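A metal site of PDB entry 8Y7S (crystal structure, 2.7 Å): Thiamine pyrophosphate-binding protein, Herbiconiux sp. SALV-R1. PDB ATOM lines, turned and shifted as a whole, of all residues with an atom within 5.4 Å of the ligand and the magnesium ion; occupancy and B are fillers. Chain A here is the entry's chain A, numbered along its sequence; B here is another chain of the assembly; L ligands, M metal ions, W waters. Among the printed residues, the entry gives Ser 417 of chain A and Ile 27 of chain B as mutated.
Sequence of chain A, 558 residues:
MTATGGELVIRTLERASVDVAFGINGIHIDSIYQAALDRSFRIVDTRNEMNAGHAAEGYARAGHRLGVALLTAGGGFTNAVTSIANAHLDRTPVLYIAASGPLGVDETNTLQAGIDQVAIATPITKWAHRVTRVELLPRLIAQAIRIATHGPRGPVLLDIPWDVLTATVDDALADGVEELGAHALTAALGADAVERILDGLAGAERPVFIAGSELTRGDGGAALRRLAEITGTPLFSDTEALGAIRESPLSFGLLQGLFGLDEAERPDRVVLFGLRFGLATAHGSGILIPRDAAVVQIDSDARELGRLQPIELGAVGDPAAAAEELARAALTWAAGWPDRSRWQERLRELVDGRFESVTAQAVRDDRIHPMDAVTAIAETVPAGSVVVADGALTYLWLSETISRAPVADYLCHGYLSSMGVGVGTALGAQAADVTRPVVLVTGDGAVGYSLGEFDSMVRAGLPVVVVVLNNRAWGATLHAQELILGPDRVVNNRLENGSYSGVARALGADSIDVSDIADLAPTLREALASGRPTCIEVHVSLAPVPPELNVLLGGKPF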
ATOM      1  N   GLY A 391     -18.331 -17.386  12.758  1.00  0.00           N
ATOM      2  CA  GLY A 391     -19.427 -16.469  13.015  1.00  0.00           C
ATOM      3  C   GLY A 391     -19.962 -15.951  11.692  1.00  0.00           C
ATOM      4  O   GLY A 391     -19.272 -16.033  10.678  1.00  0.00           O
ATOM      5  N   ALA A 392     -21.203 -15.441  11.683  1.00  0.00           N
ATOM      6  CA  ALA A 392     -21.822 -15.013  10.426  1.00  0.00           C
ATOM      7  C   ALA A 392     -21.607 -13.529  10.159  1.00  0.00           C
ATOM      8  O   ALA A 392     -20.807 -13.142   9.300  1.00  0.00           O
ATOM      9  CB  ALA A 392     -23.301 -15.376  10.423  1.00  0.00           C
ATOM     10  N   LEU A 393     -22.336 -12.667  10.890  1.00  0.00           N
ATOM     11  CA  LEU A 393     -22.119 -11.223  10.751  1.00  0.00           C
ATOM     12  C   LEU A 393     -20.651 -10.887  10.978  1.00  0.00           C
ATOM     13  O   LEU A 393     -20.115  -9.959  10.349  1.00  0.00           O
ATOM     14  CB  LEU A 393     -23.010 -10.452  11.724  1.00  0.00           C
ATOM     15  CG  LEU A 393     -24.523 -10.576  11.521  1.00  0.00           C
ATOM     16  CD1 LEU A 393     -25.302  -9.869  12.627  1.00  0.00           C
ATOM     17  CD2 LEU A 393     -24.941 -10.094  10.130  1.00  0.00           C
ATOM     18  N   THR A 394     -19.987 -11.627  11.865  1.00  0.00           N
ATOM     19  CA  THR A 394     -18.555 -11.456  12.118  1.00  0.00           C
ATOM     20  C   THR A 394     -17.733 -11.591  10.838  1.00  0.00           C
ATOM     21  O   THR A 394     -16.970 -10.693  10.478  1.00  0.00           O
ATOM     22  CB  THR A 394     -18.088 -12.457  13.170  1.00  0.00           C
ATOM     23  OG1 THR A 394     -18.764 -12.204  14.410  1.00  0.00           O
ATOM     24  CG2 THR A 394     -16.591 -12.350  13.382  1.00  0.00           C
ATOM     25  N   LEU A 416     -20.393 -24.677   2.755  1.00  0.00           N
ATOM     26  CA  LEU A 416     -21.158 -25.288   3.829  1.00  0.00           C
ATOM     27  C   LEU A 416     -21.605 -24.261   4.874  1.00  0.00           C
ATOM     28  O   LEU A 416     -22.691 -24.425   5.454  1.00  0.00           O
ATOM     29  CB  LEU A 416     -20.343 -26.393   4.505  1.00  0.00           C
ATOM     30  CG  LEU A 416     -21.132 -27.258   5.479  1.00  0.00           C
ATOM     31  CD1 LEU A 416     -22.160 -28.090   4.715  1.00  0.00           C
ATOM     32  CD2 LEU A 416     -20.206 -28.147   6.293  1.00  0.00           C
ATOM     33  N   SER A 417     -20.804 -23.226   5.127  1.00  0.00           N
ATOM     34  CA  SER A 417     -21.130 -22.172   6.083  1.00  0.00           C
ATOM     35  C   SER A 417     -21.524 -22.736   7.436  1.00  0.00           C
ATOM     36  O   SER A 417     -22.522 -22.341   8.046  1.00  0.00           O
ATOM     37  CB  SER A 417     -22.226 -21.248   5.539  1.00  0.00           C
ATOM     38  OG  SER A 417     -21.645 -20.222   4.758  1.00  0.00           O
ATOM     39  N   SER A 418     -20.746 -23.699   7.910  1.00  0.00           N
ATOM     40  CA  SER A 418     -21.067 -24.409   9.134  1.00  0.00           C
ATOM     41  C   SER A 418     -20.495 -23.630  10.313  1.00  0.00           C
ATOM     42  O   SER A 418     -19.276 -23.564  10.498  1.00  0.00           O
ATOM     43  CB  SER A 418     -20.515 -25.838   9.089  1.00  0.00           C
ATOM     44  OG  SER A 418     -20.869 -26.549  10.255  1.00  0.00           O
ATOM     45  N   MET A 419     -21.386 -23.042  11.119  1.00  0.00           N
ATOM     46  CA  MET A 419     -20.960 -22.312  12.299  1.00  0.00           C
ATOM     47  C   MET A 419     -20.269 -23.259  13.277  1.00  0.00           C
ATOM     48  O   MET A 419     -20.764 -24.361  13.543  1.00  0.00           O
ATOM     49  CB  MET A 419     -22.176 -21.645  12.959  1.00  0.00           C
ATOM     50  CG  MET A 419     -22.623 -20.317  12.309  1.00  0.00           C
ATOM     51  SD  MET A 419     -21.308 -19.300  11.609  1.00  0.00           S
ATOM     52  CE  MET A 419     -21.964 -18.872  10.020  1.00  0.00           C
ATOM     53  N   GLY A 443     -17.687 -15.439  16.226  1.00  0.00           N
ATOM     54  CA  GLY A 443     -18.853 -14.974  16.940  1.00  0.00           C
ATOM     55  C   GLY A 443     -19.091 -15.706  18.243  1.00  0.00           C
ATOM     56  O   GLY A 443     -18.474 -16.740  18.526  1.00  0.00           O
ATOM     57  N   ASP A 444     -20.004 -15.164  19.049  1.00  0.00           N
ATOM     58  CA  ASP A 444     -20.312 -15.751  20.348  1.00  0.00           C
ATOM     59  C   ASP A 444     -21.024 -17.089  20.200  1.00  0.00           C
ATOM     60  O   ASP A 444     -20.744 -18.032  20.951  1.00  0.00           O
ATOM     61  CB  ASP A 444     -21.164 -14.791  21.182  1.00  0.00           C
ATOM     62  CG  ASP A 444     -22.421 -14.317  20.449  1.00  0.00           C
ATOM     63  OD1 ASP A 444     -22.340 -13.965  19.246  1.00  0.00           O
ATOM     64  OD2 ASP A 444     -23.496 -14.309  21.089  1.00  0.00           O
ATOM     65  N   GLY A 445     -21.919 -17.204  19.225  1.00  0.00           N
ATOM     66  CA  GLY A 445     -22.598 -18.473  18.994  1.00  0.00           C
ATOM     67  C   GLY A 445     -21.645 -19.547  18.498  1.00  0.00           C
ATOM     68  O   GLY A 445     -21.628 -20.672  19.011  1.00  0.00           O
ATOM     69  N   ALA A 446     -20.814 -19.200  17.505  1.00  0.00           N
ATOM     70  CA  ALA A 446     -19.933 -20.183  16.897  1.00  0.00           C
ATOM     71  C   ALA A 446     -18.928 -20.720  17.908  1.00  0.00           C
ATOM     72  O   ALA A 446     -18.715 -21.929  17.983  1.00  0.00           O
ATOM     73  CB  ALA A 446     -19.204 -19.561  15.704  1.00  0.00           C
ATOM     74  N   VAL A 447     -18.316 -19.842  18.716  1.00  0.00           N
ATOM     75  CA  VAL A 447     -17.284 -20.288  19.643  1.00  0.00           C
ATOM     76  C   VAL A 447     -17.854 -21.246  20.689  1.00  0.00           C
ATOM     77  O   VAL A 447     -17.128 -22.072  21.240  1.00  0.00           O
ATOM     78  CB  VAL A 447     -16.584 -19.087  20.316  1.00  0.00           C
ATOM     79  CG1 VAL A 447     -17.381 -18.569  21.511  1.00  0.00           C
ATOM     80  CG2 VAL A 447     -15.172 -19.468  20.723  1.00  0.00           C
ATOM     81  N   TYR A 449     -19.555 -23.794  20.165  1.00  0.00           N
ATOM     82  CA  TYR A 449     -19.518 -25.169  19.687  1.00  0.00           C
ATOM     83  C   TYR A 449     -18.369 -25.957  20.311  1.00  0.00           C
ATOM     84  O   TYR A 449     -18.526 -27.157  20.613  1.00  0.00           O
ATOM     85  CB  TYR A 449     -19.388 -25.203  18.162  1.00  0.00           C
ATOM     86  CG  TYR A 449     -20.707 -25.186  17.418  1.00  0.00           C
ATOM     87  CD1 TYR A 449     -21.423 -26.346  17.206  1.00  0.00           C
ATOM     88  CD2 TYR A 449     -21.219 -24.001  16.921  1.00  0.00           C
ATOM     89  CE1 TYR A 449     -22.626 -26.329  16.519  1.00  0.00           C
ATOM     90  CE2 TYR A 449     -22.414 -23.972  16.235  1.00  0.00           C
ATOM     91  CZ  TYR A 449     -23.107 -25.136  16.037  1.00  0.00           C
ATOM     92  OH  TYR A 449     -24.303 -25.089  15.359  1.00  0.00           O
ATOM     93  N   LEU A 469     -16.151 -11.817  18.804  1.00  0.00           N
ATOM     94  CA  LEU A 469     -17.036 -10.665  18.639  1.00  0.00           C
ATOM     95  C   LEU A 469     -18.394 -11.041  19.215  1.00  0.00           C
ATOM     96  O   LEU A 469     -19.189 -11.710  18.567  1.00  0.00           O
ATOM     97  CB  LEU A 469     -17.152 -10.263  17.178  1.00  0.00           C
ATOM     98  CG  LEU A 469     -15.876  -9.828  16.460  1.00  0.00           C
ATOM     99  CD1 LEU A 469     -16.207  -8.835  15.356  1.00  0.00           C
ATOM    100  CD2 LEU A 469     -14.870  -9.219  17.423  1.00  0.00           C
ATOM    101  N   ASN A 470     -18.659 -10.603  20.453  1.00  0.00           N
ATOM    102  CA  ASN A 470     -19.906 -11.024  21.169  1.00  0.00           C
ATOM    103  C   ASN A 470     -21.065 -10.043  20.928  1.00  0.00           C
ATOM    104  O   ASN A 470     -21.056  -8.973  21.555  1.00  0.00           O
ATOM    105  CB  ASN A 470     -19.633 -11.189  22.652  1.00  0.00           C
ATOM    106  CG  ASN A 470     -20.753 -11.846  23.422  1.00  0.00           C
ATOM    107  OD1 ASN A 470     -21.820 -12.119  22.876  1.00  0.00           O
ATOM    108  ND2 ASN A 470     -20.523 -12.109  24.704  1.00  0.00           N
ATOM    109  N   ASN A 471     -22.008 -10.399  20.052  1.00  0.00           N
ATOM    110  CA  ASN A 471     -23.228  -9.557  19.842  1.00  0.00           C
ATOM    111  C   ASN A 471     -24.345 -10.073  20.751  1.00  0.00           C
ATOM    112  O   ASN A 471     -25.467  -9.524  20.648  1.00  0.00           O
ATOM    113  CB  ASN A 471     -23.605  -9.429  18.374  1.00  0.00           C
ATOM    114  CG  ASN A 471     -23.837 -10.751  17.692  1.00  0.00           C
ATOM    115  OD1 ASN A 471     -23.780 -11.799  18.322  1.00  0.00           O
ATOM    116  ND2 ASN A 471     -24.111 -10.713  16.393  1.00  0.00           N
ATOM    117  N   ARG A 472     -24.079 -11.112  21.547  1.00  0.00           N
ATOM    118  CA  ARG A 472     -25.083 -11.680  22.505  1.00  0.00           C
ATOM    119  C   ARG A 472     -26.269 -12.248  21.717  1.00  0.00           C
ATOM    120  O   ARG A 472     -27.402 -12.175  22.232  1.00  0.00           O
ATOM    121  CB  ARG A 472     -25.509 -10.653  23.556  1.00  0.00           C
ATOM    122  N   ALA A 473     -26.006 -12.823  20.549  1.00  0.00           N
ATOM    123  CA  ALA A 473     -27.059 -13.416  19.725  1.00  0.00           C
ATOM    124  C   ALA A 473     -26.452 -14.290  18.638  1.00  0.00           C
ATOM    125  O   ALA A 473     -25.270 -14.157  18.296  1.00  0.00           O
ATOM    126  CB  ALA A 473     -27.937 -12.322  19.085  1.00  0.00           C
ATOM    127  N   TRP A 474     -27.284 -15.192  18.101  1.00  0.00           N
ATOM    128  CA  TRP A 474     -27.050 -15.775  16.784  1.00  0.00           C
ATOM    129  C   TRP A 474     -27.340 -14.675  15.774  1.00  0.00           C
ATOM    130  O   TRP A 474     -28.496 -14.455  15.403  1.00  0.00           O
ATOM    131  CB  TRP A 474     -27.952 -16.991  16.525  1.00  0.00           C
ATOM    132  CG  TRP A 474     -27.748 -18.205  17.416  1.00  0.00           C
ATOM    133  CD1 TRP A 474     -28.573 -18.622  18.425  1.00  0.00           C
ATOM    134  CD2 TRP A 474     -26.678 -19.158  17.351  1.00  0.00           C
ATOM    135  NE1 TRP A 474     -28.074 -19.763  18.998  1.00  0.00           N
ATOM    136  CE2 TRP A 474     -26.912 -20.118  18.358  1.00  0.00           C
ATOM    137  CE3 TRP A 474     -25.550 -19.290  16.550  1.00  0.00           C
ATOM    138  CZ2 TRP A 474     -26.063 -21.196  18.571  1.00  0.00           C
ATOM    139  CZ3 TRP A 474     -24.701 -20.359  16.767  1.00  0.00           C
ATOM    140  CH2 TRP A 474     -24.962 -21.297  17.768  1.00  0.00           C
ATOM    141  N   GLY A 475     -26.305 -13.955  15.361  1.00  0.00           N
ATOM    142  CA  GLY A 475     -26.482 -12.700  14.643  1.00  0.00           C
ATOM    143  C   GLY A 475     -27.260 -12.738  13.344  1.00  0.00           C
ATOM    144  O   GLY A 475     -28.351 -12.161  13.264  1.00  0.00           O
ATOM    145  N   ALA A 476     -26.693 -13.391  12.317  1.00  0.00           N
ATOM    146  CA  ALA A 476     -27.275 -13.304  10.977  1.00  0.00           C
ATOM    147  C   ALA A 476     -28.675 -13.896  10.944  1.00  0.00           C
ATOM    148  O   ALA A 476     -29.568 -13.370  10.262  1.00  0.00           O
ATOM    149  CB  ALA A 476     -26.378 -13.990   9.957  1.00  0.00           C
ATOM    150  N   THR A 477     -28.902 -14.996  11.655  1.00  0.00           N
ATOM    151  CA  THR A 477     -30.247 -15.555  11.718  1.00  0.00           C
ATOM    152  C   THR A 477     -31.212 -14.577  12.370  1.00  0.00           C
ATOM    153  O   THR A 477     -32.347 -14.405  11.909  1.00  0.00           O
ATOM    154  CB  THR A 477     -30.229 -16.872  12.468  1.00  0.00           C
ATOM    155  OG1 THR A 477     -29.174 -16.844  13.434  1.00  0.00           O
ATOM    156  CG2 THR A 477     -29.992 -18.018  11.502  1.00  0.00           C
ATOM    157  N   ASN A 493     -33.060 -16.883  18.754  1.00  0.00           N
ATOM    158  CA  ASN A 493     -31.737 -16.479  18.287  1.00  0.00           C
ATOM    159  C   ASN A 493     -30.898 -15.679  19.268  1.00  0.00           C
ATOM    160  O   ASN A 493     -29.771 -15.304  18.932  1.00  0.00           O
ATOM    161  CB  ASN A 493     -31.865 -15.684  16.976  1.00  0.00           C
ATOM    162  CG  ASN A 493     -31.896 -16.580  15.747  1.00  0.00           C
ATOM    163  OD1 ASN A 493     -31.077 -17.489  15.613  1.00  0.00           O
ATOM    164  ND2 ASN A 493     -32.852 -16.326  14.860  1.00  0.00           N
ATOM    165  N   LEU A 495     -28.650 -14.899  22.697  1.00  0.00           N
ATOM    166  CA  LEU A 495     -27.714 -15.582  23.595  1.00  0.00           C
ATOM    167  C   LEU A 495     -27.201 -14.614  24.663  1.00  0.00           C
ATOM    168  O   LEU A 495     -26.013 -14.318  24.755  1.00  0.00           O
ATOM    169  CB  LEU A 495     -26.547 -16.212  22.830  1.00  0.00           C
ATOM    170  CG  LEU A 495     -26.912 -17.190  21.718  1.00  0.00           C
ATOM    171  CD1 LEU A 495     -25.705 -17.499  20.841  1.00  0.00           C
ATOM    172  CD2 LEU A 495     -27.474 -18.455  22.317  1.00  0.00           C
ATOM    173  N   ILE B  24     -31.302 -25.605  16.345  1.00  0.00           N
ATOM    174  CA  ILE B  24     -30.703 -24.282  16.232  1.00  0.00           C
ATOM    175  C   ILE B  24     -31.271 -23.624  14.981  1.00  0.00           C
ATOM    176  O   ILE B  24     -31.272 -24.232  13.906  1.00  0.00           O
ATOM    177  CB  ILE B  24     -29.168 -24.358  16.156  1.00  0.00           C
ATOM    178  CG1 ILE B  24     -28.597 -24.911  17.468  1.00  0.00           C
ATOM    179  CG2 ILE B  24     -28.565 -22.990  15.849  1.00  0.00           C
ATOM    180  CD1 ILE B  24     -27.098 -24.965  17.487  1.00  0.00           C
ATOM    181  N   ASN B  25     -31.746 -22.388  15.120  1.00  0.00           N
ATOM    182  CA  ASN B  25     -32.427 -21.736  14.018  1.00  0.00           C
ATOM    183  C   ASN B  25     -31.479 -21.489  12.846  1.00  0.00           C
ATOM    184  O   ASN B  25     -30.276 -21.299  13.015  1.00  0.00           O
ATOM    185  CB  ASN B  25     -33.042 -20.413  14.470  1.00  0.00           C
ATOM    186  CG  ASN B  25     -33.904 -19.760  13.397  1.00  0.00           C
ATOM    187  OD1 ASN B  25     -33.464 -18.830  12.708  1.00  0.00           O
ATOM    188  ND2 ASN B  25     -35.132 -20.233  13.251  1.00  0.00           N
ATOM    189  N   GLY B  26     -32.055 -21.501  11.645  1.00  0.00           N
ATOM    190  CA  GLY B  26     -31.345 -21.127  10.443  1.00  0.00           C
ATOM    191  C   GLY B  26     -32.366 -20.666   9.429  1.00  0.00           C
ATOM    192  O   GLY B  26     -33.565 -20.919   9.578  1.00  0.00           O
ATOM    193  N   ILE B  27     -31.890 -19.980   8.386  1.00  0.00           N
ATOM    194  CA  ILE B  27     -32.818 -19.410   7.421  1.00  0.00           C
ATOM    195  C   ILE B  27     -33.592 -20.507   6.686  1.00  0.00           C
ATOM    196  O   ILE B  27     -34.781 -20.341   6.359  1.00  0.00           O
ATOM    197  CB  ILE B  27     -32.075 -18.471   6.442  1.00  0.00           C
ATOM    198  CG1 ILE B  27     -33.054 -17.492   5.764  1.00  0.00           C
ATOM    199  CG2 ILE B  27     -31.281 -19.254   5.392  1.00  0.00           C
ATOM    200  CD1 ILE B  27     -34.069 -16.864   6.708  1.00  0.00           C
ATOM    201  N   GLU B  49     -25.824 -28.679  17.340  1.00  0.00           N
ATOM    202  CA  GLU B  49     -26.888 -29.524  16.789  1.00  0.00           C
ATOM    203  C   GLU B  49     -26.727 -30.962  17.257  1.00  0.00           C
ATOM    204  O   GLU B  49     -27.714 -31.694  17.389  1.00  0.00           O
ATOM    205  CB  GLU B  49     -26.890 -29.457  15.272  1.00  0.00           C
ATOM    206  CG  GLU B  49     -27.631 -28.267  14.729  1.00  0.00           C
ATOM    207  CD  GLU B  49     -26.701 -27.099  14.467  1.00  0.00           C
ATOM    208  OE1 GLU B  49     -25.526 -27.182  14.906  1.00  0.00           O
ATOM    209  OE2 GLU B  49     -27.131 -26.128  13.823  1.00  0.00           O
ATOM    210  N   THR B  72     -31.114 -27.414  10.628  1.00  0.00           N
ATOM    211  CA  THR B  72     -31.016 -26.597   9.429  1.00  0.00           C
ATOM    212  C   THR B  72     -30.072 -27.249   8.419  1.00  0.00           C
ATOM    213  O   THR B  72     -29.457 -28.289   8.689  1.00  0.00           O
ATOM    214  CB  THR B  72     -30.549 -25.180   9.772  1.00  0.00           C
ATOM    215  OG1 THR B  72     -30.903 -24.294   8.712  1.00  0.00           O
ATOM    216  CG2 THR B  72     -29.051 -25.137   9.982  1.00  0.00           C
ATOM    217  N   ALA B  73     -29.967 -26.667   7.240  1.00  0.00           N
ATOM    218  CA  ALA B  73     -29.251 -27.309   6.143  1.00  0.00           C
ATOM    219  C   ALA B  73     -27.758 -27.411   6.443  1.00  0.00           C
ATOM    220  O   ALA B  73     -27.201 -26.672   7.259  1.00  0.00           O
ATOM    221  CB  ALA B  73     -29.454 -26.547   4.840  1.00  0.00           C
ATOM    222  N   GLY B  75     -24.331 -28.004   7.725  1.00  0.00           N
ATOM    223  CA  GLY B  75     -23.743 -28.270   9.029  1.00  0.00           C
ATOM    224  C   GLY B  75     -24.789 -28.504  10.089  1.00  0.00           C
ATOM    225  O   GLY B  75     -24.537 -29.216  11.066  1.00  0.00           O
ATOM    226  N   GLY B  76     -25.972 -27.892   9.949  1.00  0.00           N
ATOM    227  CA  GLY B  76     -27.069 -28.214  10.836  1.00  0.00           C
ATOM    228  C   GLY B  76     -27.377 -29.694  10.855  1.00  0.00           C
ATOM    229  O   GLY B  76     -27.554 -30.300  11.912  1.00  0.00           O
ATOM    230  N   ASN B  79     -23.922 -32.092  11.920  1.00  0.00           N
ATOM    231  CA  ASN B  79     -23.605 -32.112  13.346  1.00  0.00           C
ATOM    232  C   ASN B  79     -24.488 -33.065  14.138  1.00  0.00           C
ATOM    233  O   ASN B  79     -24.117 -33.431  15.255  1.00  0.00           O
ATOM    234  CB  ASN B  79     -23.690 -30.707  13.926  1.00  0.00           C
ATOM    235  CG  ASN B  79     -22.410 -29.903  13.718  1.00  0.00           C
ATOM    236  OD1 ASN B  79     -21.359 -30.461  13.419  1.00  0.00           O
ATOM    237  ND2 ASN B  79     -22.511 -28.593  13.881  1.00  0.00           N
ATOM    238  N   GLN B 112     -24.943 -23.831   2.107  1.00  0.00           N
ATOM    239  CA  GLN B 112     -25.440 -24.943   2.910  1.00  0.00           C
ATOM    240  C   GLN B 112     -26.068 -26.046   2.067  1.00  0.00           C
ATOM    241  O   GLN B 112     -26.931 -26.786   2.547  1.00  0.00           O
ATOM    242  CB  GLN B 112     -26.436 -24.448   3.975  1.00  0.00           C
ATOM    243  CG  GLN B 112     -25.792 -23.980   5.272  1.00  0.00           C
ATOM    244  CD  GLN B 112     -26.658 -23.000   6.052  1.00  0.00           C
ATOM    245  OE1 GLN B 112     -26.438 -21.790   6.012  1.00  0.00           O
ATOM    246  NE2 GLN B 112     -27.660 -23.521   6.762  1.00  0.00           N
HETATM  247  N1  LIG L   1     -25.875 -24.423  12.205  1.00  0.00           N
HETATM  248  C1  LIG L   1     -24.802 -24.524  11.420  1.00  0.00           C
HETATM  249  C2  LIG L   1     -23.891 -25.689  11.650  1.00  0.00           C
HETATM  250  N2  LIG L   1     -24.478 -23.666  10.449  1.00  0.00           N
HETATM  251  C3  LIG L   1     -25.298 -22.623  10.248  1.00  0.00           C
HETATM  252  N3  LIG L   1     -24.976 -21.771   9.264  1.00  0.00           N
HETATM  253  C4  LIG L   1     -26.451 -22.424  11.036  1.00  0.00           C
HETATM  254  C5  LIG L   1     -26.684 -23.372  12.015  1.00  0.00           C
HETATM  255  C6  LIG L   1     -27.388 -21.253  10.838  1.00  0.00           C
HETATM  256  N4  LIG L   1     -26.760 -19.956  11.147  1.00  0.00           N
HETATM  257  C7  LIG L   1     -26.239 -19.130  10.198  1.00  0.00           C
HETATM  258  S1  LIG L   1     -25.615 -17.758  10.912  1.00  0.00           S
HETATM  259  C8  LIG L   1     -25.970 -18.188  12.481  1.00  0.00           C
HETATM  260  C9  LIG L   1     -26.624 -19.427  12.453  1.00  0.00           C
HETATM  261  C10 LIG L   1     -27.131 -20.167  13.650  1.00  0.00           C
HETATM  262  C11 LIG L   1     -25.644 -17.262  13.606  1.00  0.00           C
HETATM  263  C12 LIG L   1     -24.190 -17.277  14.004  1.00  0.00           C
HETATM  264  O1  LIG L   1     -24.066 -16.536  15.238  1.00  0.00           O
HETATM  265  P1  LIG L   1     -22.616 -16.077  15.748  1.00  0.00           P
HETATM  266  O2  LIG L   1     -22.771 -15.443  17.095  1.00  0.00           O
HETATM  267  O3  LIG L   1     -21.695 -17.239  15.624  1.00  0.00           O
HETATM  268  O4  LIG L   1     -22.205 -14.932  14.705  1.00  0.00           O
HETATM  269  P2  LIG L   1     -22.860 -13.505  14.348  1.00  0.00           P
HETATM  270  O5  LIG L   1     -23.621 -13.132  15.589  1.00  0.00           O
HETATM  271  O6  LIG L   1     -23.762 -13.707  13.155  1.00  0.00           O
HETATM  272  O7  LIG L   1     -21.717 -12.555  14.067  1.00  0.00           O
HETATM  273 MG    MG M   1     -23.116 -13.343  17.300  1.00  0.00          MG
HETATM  274  O   HOH W   1     -28.983 -19.294   8.259  1.00  0.00           O
HETATM  275  O   HOH W   2     -21.121 -12.353  17.362  1.00  0.00           O
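O2 of the ligand sits close to N of Asp 444 (3.4 Å).
The side-chain carboxylate (OE2) of Glu 49 of chain B is in hydrogen-bond range of a nitrogen (N1) of the ligand (2.7 Å).
A nitrogen (N3) of the ligand lies within hydrogen-bond range of the backbone carbonyl oxygen of Ser 417.
N of Gly 475 sits close to O6 of the ligand (3.4 Å).
N of Ala 446 is in hydrogen-bond range of O3 of the ligand (2.9 Å).
N of Leu 393 sits at hydrogen-bond distance from O6 of the ligand (2.9 Å).
The backbone NH (N) of Gly 445 sits close to an oxygen (O2) of the ligand (2.9 Å).
The backbone NH (N) of Thr 394 lies within hydrogen-bond range of an oxygen (O7) of the ligand (3.0 Å).
An oxygen (O7) of the ligand sits at hydrogen-bond distance from the side-chain hydroxyl (OG1) of Thr 394 (3.0 Å).
The backbone NH (N) of Ala 476 sits at hydrogen-bond distance from an oxygen (O6) of the ligand (3.1 Å).
N of Ala 392 is in hydrogen-bond range of O4 of the ligand, 3.2 Å away.
N2 of the ligand is in hydrogen-bond range of N of Met 419.
The side-chain carboxylate (OE1) of Glu 49 of chain B lies within hydrogen-bond range of the side-chain hydroxyl (OH) of Tyr 449 (2.5 Å).
The side-chain amide nitrogen of Asn 79 of chain B sits at hydrogen-bond distance from the side-chain carboxylate of Glu 49 of chain B (3.5 Å).
SD of Met 419 sits close to N of Gly 391.
The backbone carbonyl oxygen (O) of Trp 474 lies within hydrogen-bond range of the side-chain hydroxyl (OG1) of Thr 477.
The backbone NH of Trp 474 is in hydrogen-bond range of the backbone carbonyl oxygen of Asn 493 (2.6 Å).
The side-chain amide nitrogen of Asn 493 sits at hydrogen-bond distance from the side-chain amide oxygen of Asn 25 of chain B (3.4 Å).
The side-chain hydroxyl (OG1) of Thr 477 is in hydrogen-bond range of the side-chain amide oxygen (OD1) of Asn 493 (3.0 Å).
The side-chain amide nitrogen (NE2) of Gln 112 of chain B sits at hydrogen-bond distance from the backbone carbonyl oxygen (O) of Ala 73 of chain B, 3.2 Å away.
Residues that only touch the ligand: Gly 75 of chain B, Trp 474, Asn 25 of chain B, Ser 418, Gly 76 of chain B, Gly 391, Thr 477, Gln 112 of chain B, Thr 72 of chain B, Tyr 449, Ile 24 of chain B, Gly 443, Asn 79 of chain B and Gly 26 of chain B.
Hydrophobic or aromatic side chains that line the ligand: Ala 392, Leu 393, Met 419, Ala 446, Trp 474, Ala 476 and Ile 24 of chain B.
Of the 36 residues printed, 27 come within 4 Å of the ligand.
N of Gly 475 touches the magnesium ion (3.8 Å).
Of the 36 residues printed, 4 come within 4 Å of the magnesium ion.
Along chain A the residues within 4 Å of the magnesium ion span positions 444 to 475.
The magnesium ion is bound by O5 of the ligand (1.8 Å), OD1 of Asn 471 (2.0 Å), O2 of the ligand (2.1 Å), OD1 of Asp 444 (2.2 Å), water W2 (2.2 Å) and O of Ala 473 (2.5 Å).
Water W2 lies within hydrogen-bond range of an oxygen (O7) of the ligand (3.4 Å), the backbone NH of Asn 471 (3.4 Å) and the backbone NH of Asp 444 (3.5 Å).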
